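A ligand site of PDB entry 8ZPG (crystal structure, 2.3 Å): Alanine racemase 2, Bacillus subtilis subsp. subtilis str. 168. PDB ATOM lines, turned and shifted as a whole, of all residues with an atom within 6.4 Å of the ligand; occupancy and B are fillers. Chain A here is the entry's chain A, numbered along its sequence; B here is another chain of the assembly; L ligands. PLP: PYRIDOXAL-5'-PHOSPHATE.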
ATOM      1  N   VAL A  41      -8.610 -17.249  12.597  1.00  0.00           N
ATOM      2  CA  VAL A  41      -9.245 -18.412  11.976  1.00  0.00           C
ATOM      3  C   VAL A  41      -9.302 -19.555  13.005  1.00  0.00           C
ATOM      4  O   VAL A  41      -8.260 -20.055  13.447  1.00  0.00           O
ATOM      5  CB  VAL A  41      -8.509 -18.849  10.688  1.00  0.00           C
ATOM      6  CG1 VAL A  41      -9.334 -19.879   9.912  1.00  0.00           C
ATOM      7  CG2 VAL A  41      -8.220 -17.650   9.789  1.00  0.00           C
ATOM      8  N   LYS A  43     -11.671 -22.478  12.634  1.00  0.00           N
ATOM      9  CA  LYS A  43     -12.442 -23.583  12.098  1.00  0.00           C
ATOM     10  C   LYS A  43     -11.856 -24.927  12.553  1.00  0.00           C
ATOM     11  O   LYS A  43     -10.783 -24.988  13.163  1.00  0.00           O
ATOM     12  CB  LYS A  43     -12.468 -23.534  10.576  1.00  0.00           C
ATOM     13  CG  LYS A  43     -11.160 -23.929   9.940  1.00  0.00           C
ATOM     14  CD  LYS A  43     -10.912 -23.190   8.654  1.00  0.00           C
ATOM     15  CE  LYS A  43      -9.578 -23.621   8.017  1.00  0.00           C
ATOM     16  NZ  LYS A  43      -9.639 -23.706   6.534  1.00  0.00           N
ATOM     17  N   TYR A  47      -8.528 -25.766  15.103  1.00  0.00           N
ATOM     18  CA  TYR A  47      -7.427 -26.633  14.710  1.00  0.00           C
ATOM     19  C   TYR A  47      -7.144 -27.700  15.784  1.00  0.00           C
ATOM     20  O   TYR A  47      -5.992 -28.064  16.041  1.00  0.00           O
ATOM     21  CB  TYR A  47      -6.164 -25.830  14.397  1.00  0.00           C
ATOM     22  CG  TYR A  47      -6.212 -24.983  13.114  1.00  0.00           C
ATOM     23  CD1 TYR A  47      -7.402 -24.468  12.598  1.00  0.00           C
ATOM     24  CD2 TYR A  47      -5.027 -24.682  12.436  1.00  0.00           C
ATOM     25  CE1 TYR A  47      -7.409 -23.679  11.431  1.00  0.00           C
ATOM     26  CE2 TYR A  47      -5.018 -23.898  11.284  1.00  0.00           C
ATOM     27  CZ  TYR A  47      -6.197 -23.405  10.770  1.00  0.00           C
ATOM     28  OH  TYR A  47      -6.128 -22.647   9.612  1.00  0.00           O
ATOM     29  N   LEU A  89     -16.094 -19.435   5.293  1.00  0.00           N
ATOM     30  CA  LEU A  89     -15.125 -19.487   4.205  1.00  0.00           C
ATOM     31  C   LEU A  89     -15.488 -20.433   3.062  1.00  0.00           C
ATOM     32  O   LEU A  89     -15.134 -20.172   1.913  1.00  0.00           O
ATOM     33  CB  LEU A  89     -13.755 -19.862   4.767  1.00  0.00           C
ATOM     34  CG  LEU A  89     -13.086 -18.706   5.509  1.00  0.00           C
ATOM     35  CD1 LEU A  89     -11.993 -19.202   6.445  1.00  0.00           C
ATOM     36  CD2 LEU A  89     -12.510 -17.717   4.502  1.00  0.00           C
ATOM     37  N   ARG A 143     -10.365 -23.482  -6.300  1.00  0.00           N
ATOM     38  CA  ARG A 143     -11.269 -24.173  -5.409  1.00  0.00           C
ATOM     39  C   ARG A 143     -12.653 -23.576  -5.535  1.00  0.00           C
ATOM     40  O   ARG A 143     -13.554 -24.210  -6.101  1.00  0.00           O
ATOM     41  CB  ARG A 143     -10.755 -24.106  -3.961  1.00  0.00           C
ATOM     42  CG  ARG A 143     -11.544 -24.908  -2.910  1.00  0.00           C
ATOM     43  CD  ARG A 143     -10.777 -25.020  -1.564  1.00  0.00           C
ATOM     44  NE  ARG A 143     -10.272 -23.729  -1.068  1.00  0.00           N
ATOM     45  CZ  ARG A 143      -9.452 -23.596  -0.029  1.00  0.00           C
ATOM     46  NH1 ARG A 143      -9.026 -24.647   0.654  1.00  0.00           N
ATOM     47  NH2 ARG A 143      -9.062 -22.377   0.329  1.00  0.00           N
ATOM     48  N   PHE A 171     -12.082 -10.882  -1.199  1.00  0.00           N
ATOM     49  CA  PHE A 171     -10.778 -11.477  -0.873  1.00  0.00           C
ATOM     50  C   PHE A 171     -10.280 -12.427  -1.965  1.00  0.00           C
ATOM     51  O   PHE A 171     -10.986 -12.732  -2.935  1.00  0.00           O
ATOM     52  CB  PHE A 171     -10.832 -12.206   0.476  1.00  0.00           C
ATOM     53  CG  PHE A 171     -11.798 -13.365   0.523  1.00  0.00           C
ATOM     54  CD1 PHE A 171     -13.178 -13.160   0.675  1.00  0.00           C
ATOM     55  CD2 PHE A 171     -11.334 -14.675   0.469  1.00  0.00           C
ATOM     56  CE1 PHE A 171     -14.062 -14.231   0.781  1.00  0.00           C
ATOM     57  CE2 PHE A 171     -12.218 -15.756   0.557  1.00  0.00           C
ATOM     58  CZ  PHE A 171     -13.580 -15.524   0.707  1.00  0.00           C
ATOM     59  N   THR A 172      -9.048 -12.912  -1.785  1.00  0.00           N
ATOM     60  CA  THR A 172      -8.459 -13.973  -2.592  1.00  0.00           C
ATOM     61  C   THR A 172      -7.601 -14.860  -1.679  1.00  0.00           C
ATOM     62  O   THR A 172      -7.550 -14.662  -0.455  1.00  0.00           O
ATOM     63  CB  THR A 172      -7.661 -13.396  -3.768  1.00  0.00           C
ATOM     64  OG1 THR A 172      -7.471 -14.410  -4.749  1.00  0.00           O
ATOM     65  CG2 THR A 172      -6.291 -12.864  -3.348  1.00  0.00           C
ATOM     66  N   HIS A 173      -6.908 -15.851  -2.266  1.00  0.00           N
ATOM     67  CA  HIS A 173      -6.113 -16.830  -1.523  1.00  0.00           C
ATOM     68  C   HIS A 173      -4.903 -17.321  -2.340  1.00  0.00           C
ATOM     69  O   HIS A 173      -5.064 -17.766  -3.489  1.00  0.00           O
ATOM     70  CB  HIS A 173      -7.006 -18.011  -1.104  1.00  0.00           C
ATOM     71  CG  HIS A 173      -6.491 -18.750   0.086  1.00  0.00           C
ATOM     72  ND1 HIS A 173      -6.484 -18.211   1.358  1.00  0.00           N
ATOM     73  CD2 HIS A 173      -5.939 -19.993   0.195  1.00  0.00           C
ATOM     74  CE1 HIS A 173      -5.926 -19.071   2.193  1.00  0.00           C
ATOM     75  NE2 HIS A 173      -5.614 -20.164   1.527  1.00  0.00           N
ATOM     76  N   CYS A 212      -3.978 -12.120   2.666  1.00  0.00           N
ATOM     77  CA  CYS A 212      -2.865 -12.865   3.261  1.00  0.00           C
ATOM     78  C   CYS A 212      -3.309 -13.922   4.267  1.00  0.00           C
ATOM     79  O   CYS A 212      -4.279 -13.745   4.998  1.00  0.00           O
ATOM     80  CB  CYS A 212      -1.914 -11.914   4.008  1.00  0.00           C
ATOM     81  SG  CYS A 212      -0.874 -10.881   2.968  1.00  0.00           S
ATOM     82  N   ASN A 213      -2.543 -15.029   4.335  1.00  0.00           N
ATOM     83  CA  ASN A 213      -2.560 -16.056   5.381  1.00  0.00           C
ATOM     84  C   ASN A 213      -1.295 -15.920   6.248  1.00  0.00           C
ATOM     85  O   ASN A 213      -0.500 -14.979   6.073  1.00  0.00           O
ATOM     86  CB  ASN A 213      -2.699 -17.470   4.779  1.00  0.00           C
ATOM     87  CG  ASN A 213      -1.583 -17.809   3.779  1.00  0.00           C
ATOM     88  OD1 ASN A 213      -0.659 -17.013   3.555  1.00  0.00           O
ATOM     89  ND2 ASN A 213      -1.679 -18.986   3.160  1.00  0.00           N
ATOM     90  N   THR A 214      -1.069 -16.885   7.158  1.00  0.00           N
ATOM     91  CA  THR A 214       0.110 -16.832   8.021  1.00  0.00           C
ATOM     92  C   THR A 214       1.391 -16.626   7.206  1.00  0.00           C
ATOM     93  O   THR A 214       2.177 -15.716   7.496  1.00  0.00           O
ATOM     94  CB  THR A 214       0.239 -18.115   8.864  1.00  0.00           C
ATOM     95  OG1 THR A 214      -0.962 -18.343   9.603  1.00  0.00           O
ATOM     96  CG2 THR A 214       1.437 -18.017   9.874  1.00  0.00           C
ATOM     97  N   ALA A 215       1.635 -17.488   6.200  1.00  0.00           N
ATOM     98  CA  ALA A 215       2.884 -17.429   5.455  1.00  0.00           C
ATOM     99  C   ALA A 215       2.990 -16.134   4.664  1.00  0.00           C
ATOM    100  O   ALA A 215       4.051 -15.500   4.619  1.00  0.00           O
ATOM    101  CB  ALA A 215       3.025 -18.631   4.519  1.00  0.00           C
ATOM    102  N   ARG A 229      -5.721 -12.828   7.596  1.00  0.00           N
ATOM    103  CA  ARG A 229      -6.338 -13.992   8.251  1.00  0.00           C
ATOM    104  C   ARG A 229      -5.247 -14.858   8.901  1.00  0.00           C
ATOM    105  O   ARG A 229      -4.515 -15.574   8.207  1.00  0.00           O
ATOM    106  CB  ARG A 229      -7.152 -14.819   7.235  1.00  0.00           C
ATOM    107  CG  ARG A 229      -8.129 -13.985   6.379  1.00  0.00           C
ATOM    108  CD  ARG A 229      -8.921 -14.778   5.300  1.00  0.00           C
ATOM    109  NE  ARG A 229      -8.114 -15.361   4.225  1.00  0.00           N
ATOM    110  CZ  ARG A 229      -7.759 -14.778   3.079  1.00  0.00           C
ATOM    111  NH1 ARG A 229      -8.061 -13.512   2.821  1.00  0.00           N
ATOM    112  NH2 ARG A 229      -7.074 -15.463   2.180  1.00  0.00           N
ATOM    113  N   LEU A 230      -5.160 -14.836  10.225  1.00  0.00           N
ATOM    114  CA  LEU A 230      -4.146 -15.549  10.993  1.00  0.00           C
ATOM    115  C   LEU A 230      -4.676 -16.903  11.448  1.00  0.00           C
ATOM    116  O   LEU A 230      -5.607 -16.968  12.261  1.00  0.00           O
ATOM    117  CB  LEU A 230      -3.701 -14.705  12.208  1.00  0.00           C
ATOM    118  CG  LEU A 230      -2.575 -15.238  13.098  1.00  0.00           C
ATOM    119  CD1 LEU A 230      -1.333 -15.482  12.270  1.00  0.00           C
ATOM    120  CD2 LEU A 230      -2.270 -14.299  14.218  1.00  0.00           C
ATOM    121  N   GLY A 231      -4.089 -17.984  10.951  1.00  0.00           N
ATOM    122  CA  GLY A 231      -4.523 -19.325  11.314  1.00  0.00           C
ATOM    123  C   GLY A 231      -3.516 -20.131  12.109  1.00  0.00           C
ATOM    124  O   GLY A 231      -3.514 -20.083  13.346  1.00  0.00           O
ATOM    125  N   ILE A 232      -2.631 -20.864  11.410  1.00  0.00           N
ATOM    126  CA  ILE A 232      -1.723 -21.800  12.067  1.00  0.00           C
ATOM    127  C   ILE A 232      -0.765 -21.085  13.016  1.00  0.00           C
ATOM    128  O   ILE A 232      -0.306 -21.683  14.008  1.00  0.00           O
ATOM    129  CB  ILE A 232      -0.980 -22.653  11.014  1.00  0.00           C
ATOM    130  CG1 ILE A 232      -0.140 -23.752  11.678  1.00  0.00           C
ATOM    131  CG2 ILE A 232      -0.101 -21.808  10.082  1.00  0.00           C
ATOM    132  CD1 ILE A 232      -0.894 -25.099  11.865  1.00  0.00           C
ATOM    133  N   GLY A 233      -0.453 -19.809  12.764  1.00  0.00           N
ATOM    134  CA  GLY A 233       0.498 -19.078  13.600  1.00  0.00           C
ATOM    135  C   GLY A 233      -0.066 -18.632  14.937  1.00  0.00           C
ATOM    136  O   GLY A 233       0.694 -18.399  15.882  1.00  0.00           O
ATOM    137  N   PRO A 239       4.146 -22.489   9.103  1.00  0.00           N
ATOM    138  CA  PRO A 239       3.525 -23.112   7.926  1.00  0.00           C
ATOM    139  C   PRO A 239       4.420 -24.105   7.201  1.00  0.00           C
ATOM    140  O   PRO A 239       3.920 -25.065   6.622  1.00  0.00           O
ATOM    141  CB  PRO A 239       3.172 -21.931   7.013  1.00  0.00           C
ATOM    142  CG  PRO A 239       3.474 -20.710   7.779  1.00  0.00           C
ATOM    143  CD  PRO A 239       3.953 -21.037   9.138  1.00  0.00           C
ATOM    144  N   TYR A 368      -0.431 -29.427  10.464  1.00  0.00           N
ATOM    145  CA  TYR A 368      -1.863 -29.166  10.342  1.00  0.00           C
ATOM    146  C   TYR A 368      -2.737 -30.411  10.614  1.00  0.00           C
ATOM    147  O   TYR A 368      -3.729 -30.330  11.341  1.00  0.00           O
ATOM    148  CB  TYR A 368      -2.194 -28.648   8.941  1.00  0.00           C
ATOM    149  CG  TYR A 368      -1.751 -27.234   8.516  1.00  0.00           C
ATOM    150  CD1 TYR A 368      -0.427 -26.983   8.126  1.00  0.00           C
ATOM    151  CD2 TYR A 368      -2.688 -26.180   8.423  1.00  0.00           C
ATOM    152  CE1 TYR A 368      -0.030 -25.697   7.678  1.00  0.00           C
ATOM    153  CE2 TYR A 368      -2.309 -24.910   7.994  1.00  0.00           C
ATOM    154  CZ  TYR A 368      -0.976 -24.672   7.624  1.00  0.00           C
ATOM    155  OH  TYR A 368      -0.604 -23.407   7.175  1.00  0.00           O
ATOM    156  N   TYR B 276      -3.216 -26.435  -3.177  1.00  0.00           N
ATOM    157  CA  TYR B 276      -1.934 -26.044  -2.602  1.00  0.00           C
ATOM    158  C   TYR B 276      -0.793 -26.807  -3.271  1.00  0.00           C
ATOM    159  O   TYR B 276      -0.924 -27.982  -3.616  1.00  0.00           O
ATOM    160  CB  TYR B 276      -1.882 -26.311  -1.083  1.00  0.00           C
ATOM    161  CG  TYR B 276      -2.798 -25.441  -0.222  1.00  0.00           C
ATOM    162  CD1 TYR B 276      -2.598 -24.056  -0.093  1.00  0.00           C
ATOM    163  CD2 TYR B 276      -3.862 -26.008   0.487  1.00  0.00           C
ATOM    164  CE1 TYR B 276      -3.452 -23.275   0.696  1.00  0.00           C
ATOM    165  CE2 TYR B 276      -4.714 -25.244   1.273  1.00  0.00           C
ATOM    166  CZ  TYR B 276      -4.511 -23.886   1.383  1.00  0.00           C
ATOM    167  OH  TYR B 276      -5.378 -23.160   2.179  1.00  0.00           O
ATOM    168  N   MET B 324      -8.013 -28.916   4.349  1.00  0.00           N
ATOM    169  CA  MET B 324      -8.590 -29.181   5.672  1.00  0.00           C
ATOM    170  C   MET B 324     -10.091 -29.491   5.580  1.00  0.00           C
ATOM    171  O   MET B 324     -10.593 -30.373   6.289  1.00  0.00           O
ATOM    172  CB  MET B 324      -8.334 -28.001   6.608  1.00  0.00           C
ATOM    173  CG  MET B 324      -8.922 -28.130   8.015  1.00  0.00           C
ATOM    174  SD  MET B 324      -8.162 -27.078   9.326  1.00  0.00           S
ATOM    175  CE  MET B 324      -6.445 -27.585   9.350  1.00  0.00           C
ATOM    176  N   ASP B 325     -10.819 -28.798   4.691  1.00  0.00           N
ATOM    177  CA  ASP B 325     -12.269 -28.871   4.652  1.00  0.00           C
ATOM    178  C   ASP B 325     -12.846 -29.172   3.273  1.00  0.00           C
ATOM    179  O   ASP B 325     -14.072 -29.226   3.144  1.00  0.00           O
ATOM    180  CB  ASP B 325     -12.913 -27.563   5.144  1.00  0.00           C
ATOM    181  CG  ASP B 325     -12.396 -27.115   6.494  1.00  0.00           C
ATOM    182  OD1 ASP B 325     -12.414 -27.921   7.452  1.00  0.00           O
ATOM    183  OD2 ASP B 325     -12.000 -25.936   6.623  1.00  0.00           O
HETATM  184  N1  PLP L   1      -7.583 -18.045   4.844  1.00  0.00           N
HETATM  185  C2  PLP L   1      -8.148 -19.065   4.180  1.00  0.00           C
HETATM  186  C2A PLP L   1      -9.060 -18.777   2.969  1.00  0.00           C
HETATM  187  C3  PLP L   1      -7.896 -20.403   4.544  1.00  0.00           C
HETATM  188  O3  PLP L   1      -8.448 -21.518   3.854  1.00  0.00           O
HETATM  189  C4  PLP L   1      -7.057 -20.612   5.627  1.00  0.00           C
HETATM  190  C4A PLP L   1      -6.737 -22.053   6.064  1.00  0.00           C
HETATM  191  C5  PLP L   1      -6.511 -19.510   6.312  1.00  0.00           C
HETATM  192  C6  PLP L   1      -6.779 -18.220   5.883  1.00  0.00           C
HETATM  193  C5A PLP L   1      -5.573 -19.789   7.474  1.00  0.00           C
HETATM  194  O4P PLP L   1      -4.533 -20.450   6.812  1.00  0.00           O
HETATM  195  P   PLP L   1      -3.110 -20.663   7.584  1.00  0.00           P
HETATM  196  O1P PLP L   1      -2.077 -21.238   6.644  1.00  0.00           O
HETATM  197  O2P PLP L   1      -3.377 -21.684   8.672  1.00  0.00           O
HETATM  198  O3P PLP L   1      -2.669 -19.352   8.204  1.00  0.00           O
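N of Gly 231 lies within hydrogen-bond range of OG1 of Thr 214 (3.4 Å).
ND1 of His 173 sits at hydrogen-bond distance from NH2 of Arg 229 (2.9 Å).
The backbone carbonyl oxygen (O) of Cys 212 lies within hydrogen-bond range of the backbone NH (N) of Arg 229 (3.1 Å).
NH2 of Arg 229 sits at hydrogen-bond distance from O of Thr 172.
A ring nitrogen (NE2) of His 173 lies within hydrogen-bond range of the side-chain hydroxyl (OH) of Tyr 276 of chain B.
NZ of Lys 43 lies within salt-bridge range of OD2 of Asp 325 of chain B, at 3.2 Å.
The backbone NH of Thr 214 is in hydrogen-bond range of an oxygen (O3P) of the ligand, at 3.1 Å.
OG1 of Thr 214 is in hydrogen-bond range of O3P of the ligand.
An oxygen (O1P) of the ligand sits at hydrogen-bond distance from the side-chain hydroxyl of Tyr 368 (2.7 Å).
NE of Arg 229 lies within hydrogen-bond range of N1 of the ligand, at 2.8 Å.
The backbone NH of Ile 232 lies within hydrogen-bond range of an oxygen (O2P) of the ligand, 3.0 Å away.
OH of Tyr 47 lies within hydrogen-bond range of O2P of the ligand.
O3P of the ligand lies within hydrogen-bond range of N of Gly 231 (3.4 Å).
Merely in contact with the ligand: Lys 43 (3.4 Å), Leu 89 (3.9 Å), Arg 143 (3.7 Å), His 173 (3.0 Å), Asn 213 (3.9 Å) and Tyr 276 of chain B (3.9 Å).
Hydrophobic or aromatic side chains within 4 Å of the ligand: Tyr 47, Leu 89, His 173, Ile 232 and Tyr 368.
12 residues have an atom within 4 Å of the ligand: Lys 43, Tyr 47, Leu 89, Arg 143, His 173, Asn 213, Thr 214, Arg 229, Gly 231, Ile 232, Tyr 368 and Tyr 276 of chain B.
Along chain A the residues within 4 Å of the ligand span positions 43 to 368.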
